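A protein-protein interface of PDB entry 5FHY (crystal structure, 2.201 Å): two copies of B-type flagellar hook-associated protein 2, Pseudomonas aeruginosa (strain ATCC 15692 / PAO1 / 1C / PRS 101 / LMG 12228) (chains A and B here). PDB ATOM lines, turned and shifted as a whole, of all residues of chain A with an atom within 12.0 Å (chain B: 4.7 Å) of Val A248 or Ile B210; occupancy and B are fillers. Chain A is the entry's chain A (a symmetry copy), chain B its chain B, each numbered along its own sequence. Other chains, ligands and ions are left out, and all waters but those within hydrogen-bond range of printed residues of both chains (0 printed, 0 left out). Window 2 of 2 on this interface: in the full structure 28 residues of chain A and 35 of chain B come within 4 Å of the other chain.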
ATOM      1  N   VAL A 244     -13.452  14.169 -22.549  1.00  0.00           N
ATOM      2  CA  VAL A 244     -12.469  14.064 -23.621  1.00  0.00           C
ATOM      3  C   VAL A 244     -11.136  13.615 -23.013  1.00  0.00           C
ATOM      4  O   VAL A 244     -10.626  14.261 -22.098  1.00  0.00           O
ATOM      5  CB  VAL A 244     -12.298  15.407 -24.366  1.00  0.00           C
ATOM      6  CG1 VAL A 244     -11.370  15.243 -25.557  1.00  0.00           C
ATOM      7  CG2 VAL A 244     -13.651  15.933 -24.823  1.00  0.00           C
ATOM      8  N   VAL A 245     -10.575  12.514 -23.508  1.00  0.00           N
ATOM      9  CA  VAL A 245      -9.381  11.931 -22.890  1.00  0.00           C
ATOM     10  C   VAL A 245      -8.226  11.770 -23.879  1.00  0.00           C
ATOM     11  O   VAL A 245      -8.436  11.455 -25.052  1.00  0.00           O
ATOM     12  CB  VAL A 245      -9.703  10.543 -22.265  1.00  0.00           C
ATOM     13  CG1 VAL A 245     -10.282   9.601 -23.310  1.00  0.00           C
ATOM     14  CG2 VAL A 245      -8.467   9.926 -21.613  1.00  0.00           C
ATOM     15  N   THR A 246      -7.007  12.012 -23.401  1.00  0.00           N
ATOM     16  CA  THR A 246      -5.825  11.947 -24.249  1.00  0.00           C
ATOM     17  C   THR A 246      -4.841  10.924 -23.710  1.00  0.00           C
ATOM     18  O   THR A 246      -4.805  10.697 -22.503  1.00  0.00           O
ATOM     19  CB  THR A 246      -5.086  13.286 -24.311  1.00  0.00           C
ATOM     20  OG1 THR A 246      -6.024  14.357 -24.278  1.00  0.00           O
ATOM     21  CG2 THR A 246      -4.251  13.378 -25.571  1.00  0.00           C
ATOM     22  N   LYS A 247      -4.084  10.284 -24.598  1.00  0.00           N
ATOM     23  CA  LYS A 247      -2.699   9.917 -24.294  1.00  0.00           C
ATOM     24  C   LYS A 247      -2.035   9.344 -25.547  1.00  0.00           C
ATOM     25  O   LYS A 247      -2.706   8.772 -26.405  1.00  0.00           O
ATOM     26  CB  LYS A 247      -2.595   8.933 -23.115  1.00  0.00           C
ATOM     27  CG  LYS A 247      -1.252   8.220 -23.007  1.00  0.00           C
ATOM     28  CD  LYS A 247      -0.825   8.027 -21.559  1.00  0.00           C
ATOM     29  CE  LYS A 247       0.585   7.453 -21.478  1.00  0.00           C
ATOM     30  NZ  LYS A 247       0.807   6.359 -22.465  1.00  0.00           N
ATOM     31  N   VAL A 248      -0.720   9.512 -25.642  1.00  0.00           N
ATOM     32  CA  VAL A 248       0.078   9.052 -26.776  1.00  0.00           C
ATOM     33  C   VAL A 248      -0.124   7.576 -27.137  1.00  0.00           C
ATOM     34  O   VAL A 248      -0.651   6.793 -26.347  1.00  0.00           O
ATOM     35  CB  VAL A 248       1.575   9.275 -26.511  1.00  0.00           C
ATOM     36  CG1 VAL A 248       1.818  10.688 -26.011  1.00  0.00           C
ATOM     37  CG2 VAL A 248       2.099   8.238 -25.523  1.00  0.00           C
ATOM     38  N   GLY A 249       0.286   7.214 -28.347  1.00  0.00           N
ATOM     39  CA  GLY A 249       0.174   5.843 -28.814  1.00  0.00           C
ATOM     40  C   GLY A 249       1.312   5.449 -29.737  1.00  0.00           C
ATOM     41  O   GLY A 249       1.122   4.689 -30.687  1.00  0.00           O
ATOM     42  N   ASP B  21       3.483  10.479 -21.932  1.00  0.00           N
ATOM     43  CA  ASP B  21       4.404   9.561 -21.270  1.00  0.00           C
ATOM     44  C   ASP B  21       5.700  10.248 -20.830  1.00  0.00           C
ATOM     45  O   ASP B  21       5.707  11.022 -19.874  1.00  0.00           O
ATOM     46  CB  ASP B  21       4.708   8.365 -22.182  1.00  0.00           C
ATOM     47  CG  ASP B  21       5.087   8.780 -23.594  1.00  0.00           C
ATOM     48  OD1 ASP B  21       4.959   9.981 -23.912  1.00  0.00           O
ATOM     49  OD2 ASP B  21       5.520   7.909 -24.379  1.00  0.00           O
ATOM     50  N   LEU B  23       7.878  11.899 -23.017  1.00  0.00           N
ATOM     51  CA  LEU B  23       8.245  13.001 -23.901  1.00  0.00           C
ATOM     52  C   LEU B  23       7.230  14.136 -23.822  1.00  0.00           C
ATOM     53  O   LEU B  23       7.568  15.307 -24.009  1.00  0.00           O
ATOM     54  CB  LEU B  23       8.368  12.516 -25.348  1.00  0.00           C
ATOM     55  CG  LEU B  23       9.189  11.251 -25.611  1.00  0.00           C
ATOM     56  CD1 LEU B  23       9.267  10.972 -27.103  1.00  0.00           C
ATOM     57  CD2 LEU B  23      10.581  11.345 -25.000  1.00  0.00           C
ATOM     58  N   LYS B  24       5.983  13.772 -23.547  1.00  0.00           N
ATOM     59  CA  LYS B  24       4.871  14.703 -23.603  1.00  0.00           C
ATOM     60  C   LYS B  24       3.694  14.145 -22.818  1.00  0.00           C
ATOM     61  O   LYS B  24       3.283  13.004 -23.023  1.00  0.00           O
ATOM     62  CB  LYS B  24       4.483  14.950 -25.065  1.00  0.00           C
ATOM     63  CG  LYS B  24       3.223  15.764 -25.307  1.00  0.00           C
ATOM     64  CD  LYS B  24       2.864  15.696 -26.787  1.00  0.00           C
ATOM     65  CE  LYS B  24       2.876  14.247 -27.266  1.00  0.00           C
ATOM     66  NZ  LYS B  24       3.009  14.101 -28.740  1.00  0.00           N
ATOM     67  N   TYR B  36      -2.750  12.629 -34.287  1.00  0.00           N
ATOM     68  CA  TYR B  36      -1.737  13.602 -34.672  1.00  0.00           C
ATOM     69  C   TYR B  36      -0.336  13.026 -34.551  1.00  0.00           C
ATOM     70  O   TYR B  36       0.000  12.377 -33.562  1.00  0.00           O
ATOM     71  CB  TYR B  36      -1.848  14.865 -33.813  1.00  0.00           C
ATOM     72  CG  TYR B  36      -3.221  15.502 -33.823  1.00  0.00           C
ATOM     73  CD1 TYR B  36      -3.576  16.413 -34.812  1.00  0.00           C
ATOM     74  CD2 TYR B  36      -4.160  15.197 -32.839  1.00  0.00           C
ATOM     75  CE1 TYR B  36      -4.825  17.001 -34.828  1.00  0.00           C
ATOM     76  CE2 TYR B  36      -5.416  15.780 -32.847  1.00  0.00           C
ATOM     77  CZ  TYR B  36      -5.743  16.683 -33.845  1.00  0.00           C
ATOM     78  OH  TYR B  36      -6.988  17.272 -33.864  1.00  0.00           O
ATOM     79  N   GLN B  37       0.480  13.269 -35.568  1.00  0.00           N
ATOM     80  CA  GLN B  37       1.875  12.875 -35.518  1.00  0.00           C
ATOM     81  C   GLN B  37       2.702  14.058 -35.042  1.00  0.00           C
ATOM     82  O   GLN B  37       2.690  15.129 -35.654  1.00  0.00           O
ATOM     83  CB  GLN B  37       2.349  12.387 -36.884  1.00  0.00           C
ATOM     84  CG  GLN B  37       1.648  11.121 -37.349  1.00  0.00           C
ATOM     85  CD  GLN B  37       1.953   9.930 -36.464  1.00  0.00           C
ATOM     86  OE1 GLN B  37       1.156   9.566 -35.598  1.00  0.00           O
ATOM     87  NE2 GLN B  37       3.107   9.311 -36.682  1.00  0.00           N
ATOM     88  N   ILE B  38       3.436  13.854 -33.957  1.00  0.00           N
ATOM     89  CA  ILE B  38       4.105  14.956 -33.290  1.00  0.00           C
ATOM     90  C   ILE B  38       5.602  14.724 -33.173  1.00  0.00           C
ATOM     91  O   ILE B  38       6.047  13.648 -32.781  1.00  0.00           O
ATOM     92  CB  ILE B  38       3.516  15.186 -31.882  1.00  0.00           C
ATOM     93  CG1 ILE B  38       2.012  15.447 -31.972  1.00  0.00           C
ATOM     94  CG2 ILE B  38       4.217  16.340 -31.181  1.00  0.00           C
ATOM     95  CD1 ILE B  38       1.414  16.021 -30.710  1.00  0.00           C
ATOM     96  N   THR B 204      11.813  14.302 -29.455  1.00  0.00           N
ATOM     97  CA  THR B 204      11.600  13.025 -30.130  1.00  0.00           C
ATOM     98  C   THR B 204      12.826  12.705 -30.981  1.00  0.00           C
ATOM     99  O   THR B 204      13.517  13.608 -31.441  1.00  0.00           O
ATOM    100  CB  THR B 204      10.346  13.041 -31.024  1.00  0.00           C
ATOM    101  OG1 THR B 204      10.527  13.983 -32.088  1.00  0.00           O
ATOM    102  CG2 THR B 204       9.115  13.416 -30.216  1.00  0.00           C
ATOM    103  N   LYS B 208      11.399   9.657 -35.610  1.00  0.00           N
ATOM    104  CA  LYS B 208      10.550   8.805 -34.773  1.00  0.00           C
ATOM    105  C   LYS B 208       9.479   9.631 -34.063  1.00  0.00           C
ATOM    106  O   LYS B 208       9.661  10.023 -32.910  1.00  0.00           O
ATOM    107  CB  LYS B 208      11.333   8.010 -33.708  1.00  0.00           C
ATOM    108  CG  LYS B 208      12.424   7.019 -34.143  1.00  0.00           C
ATOM    109  CD  LYS B 208      13.595   7.593 -34.906  1.00  0.00           C
ATOM    110  CE  LYS B 208      14.716   6.559 -34.949  1.00  0.00           C
ATOM    111  NZ  LYS B 208      16.068   7.147 -35.151  1.00  0.00           N
ATOM    112  N   PRO B 209       8.363   9.912 -34.752  1.00  0.00           N
ATOM    113  CA  PRO B 209       7.372  10.833 -34.191  1.00  0.00           C
ATOM    114  C   PRO B 209       6.389  10.126 -33.259  1.00  0.00           C
ATOM    115  O   PRO B 209       6.168   8.921 -33.384  1.00  0.00           O
ATOM    116  CB  PRO B 209       6.656  11.361 -35.431  1.00  0.00           C
ATOM    117  CG  PRO B 209       6.711  10.214 -36.378  1.00  0.00           C
ATOM    118  CD  PRO B 209       8.043   9.546 -36.144  1.00  0.00           C
ATOM    119  N   ILE B 210       5.815  10.878 -32.329  1.00  0.00           N
ATOM    120  CA  ILE B 210       4.821  10.342 -31.409  1.00  0.00           C
ATOM    121  C   ILE B 210       3.423  10.402 -32.022  1.00  0.00           C
ATOM    122  O   ILE B 210       3.064  11.393 -32.658  1.00  0.00           O
ATOM    123  CB  ILE B 210       4.836  11.114 -30.067  1.00  0.00           C
ATOM    124  CG1 ILE B 210       6.202  10.991 -29.395  1.00  0.00           C
ATOM    125  CG2 ILE B 210       3.765  10.597 -29.131  1.00  0.00           C
ATOM    126  CD1 ILE B 210       6.577   9.574 -29.050  1.00  0.00           C
ATOM    127  N   THR B 211       2.636   9.346 -31.839  1.00  0.00           N
ATOM    128  CA  THR B 211       1.227   9.392 -32.215  1.00  0.00           C
ATOM    129  C   THR B 211       0.394   9.854 -31.026  1.00  0.00           C
ATOM    130  O   THR B 211       0.446   9.252 -29.954  1.00  0.00           O
ATOM    131  CB  THR B 211       0.713   8.017 -32.693  1.00  0.00           C
ATOM    132  OG1 THR B 211       1.476   7.586 -33.826  1.00  0.00           O
ATOM    133  CG2 THR B 211      -0.756   8.102 -33.086  1.00  0.00           C
ATOM    134  N   LEU B 212      -0.379  10.919 -31.219  1.00  0.00           N
ATOM    135  CA  LEU B 212      -1.233  11.434 -30.154  1.00  0.00           C
ATOM    136  C   LEU B 212      -2.708  11.263 -30.501  1.00  0.00           C
ATOM    137  O   LEU B 212      -3.186  11.795 -31.502  1.00  0.00           O
ATOM    138  CB  LEU B 212      -0.937  12.907 -29.881  1.00  0.00           C
ATOM    139  CG  LEU B 212      -1.825  13.537 -28.807  1.00  0.00           C
ATOM    140  CD1 LEU B 212      -1.273  13.177 -27.434  1.00  0.00           C
ATOM    141  CD2 LEU B 212      -1.937  15.044 -28.983  1.00  0.00           C
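O of Thr B211 sits at hydrogen-bond distance from N of Gly A249, at 2.6 Å.
O of Tyr B36 is in hydrogen-bond range of N of Leu B212, 2.8 Å away. OE1 of Gln B37 sits at hydrogen-bond distance from OG1 of Thr B211 (2.7 Å). N of Ile B38 is in hydrogen-bond range of O of Ile B210 (2.8 Å).
Among the printed residues, merely in contact across the chains: Val A248 with Thr B211 (3.2 Å), Thr A246 with Leu B212 (3.5 Å), Val A248 with Asp B21 (3.6 Å), Val A248 with Ile B210 (3.7 Å) and Val A248 with Lys B24 (3.9 Å).
Of chain B, only Asp B21, Lys B24, Ile B210 and Thr B211 come within 4 Å of Val A248. Of chain A, only Val A248 (3.7 Å) comes within 4 Å of Ile B210. Asp B21 touches one residue of chain A. No residue of chain A comes within 4 Å of Leu B23. Lys B24 touches one residue of chain A. No residue of chain A comes within 4 Å of Gln B37. No residue of chain A comes within 4 Å of Ile B38. No residue of chain A comes within 4 Å of Pro B209. Of chain A, only Val A248 (3.2 Å) and Gly A249 (2.6 Å) come within 4 Å of Thr B211. Leu B212 touches just one residue of chain A: Thr A246 (3.5 Å). Of the printed residues of chain B, Thr A246 touches Leu B212 (3.5 Å). Printed residues of chain B within 4 Å of Gly A249: Thr B211. Lys A247 touches none of the printed residues of chain B. The nearest residue of chain B that does not touch Val A248 is Leu B212 (4.1 Å). The nearest residue of chain A that does not touch Ile B210 is Gly A249 (4.9 Å).
Printed residues of chain A that touch a printed residue of chain B: Thr A246, Val A248 and Gly A249. Of the 12 printed residues of chain B, 5 touch a printed residue of chain A. Printed residues of chain B that touch a printed residue of chain A: Asp B21, Lys B24, Ile B210, Thr B211 and Leu B212. Among the printed residues, no Asp or Glu carboxylate lies within 4 Å of a Lys or Arg side-chain nitrogen of the other chain.
No position is printed for both chains. Of the 6 pairs that touch across the chains among the printed residues, none has its exchanged pair printed and touching as well.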
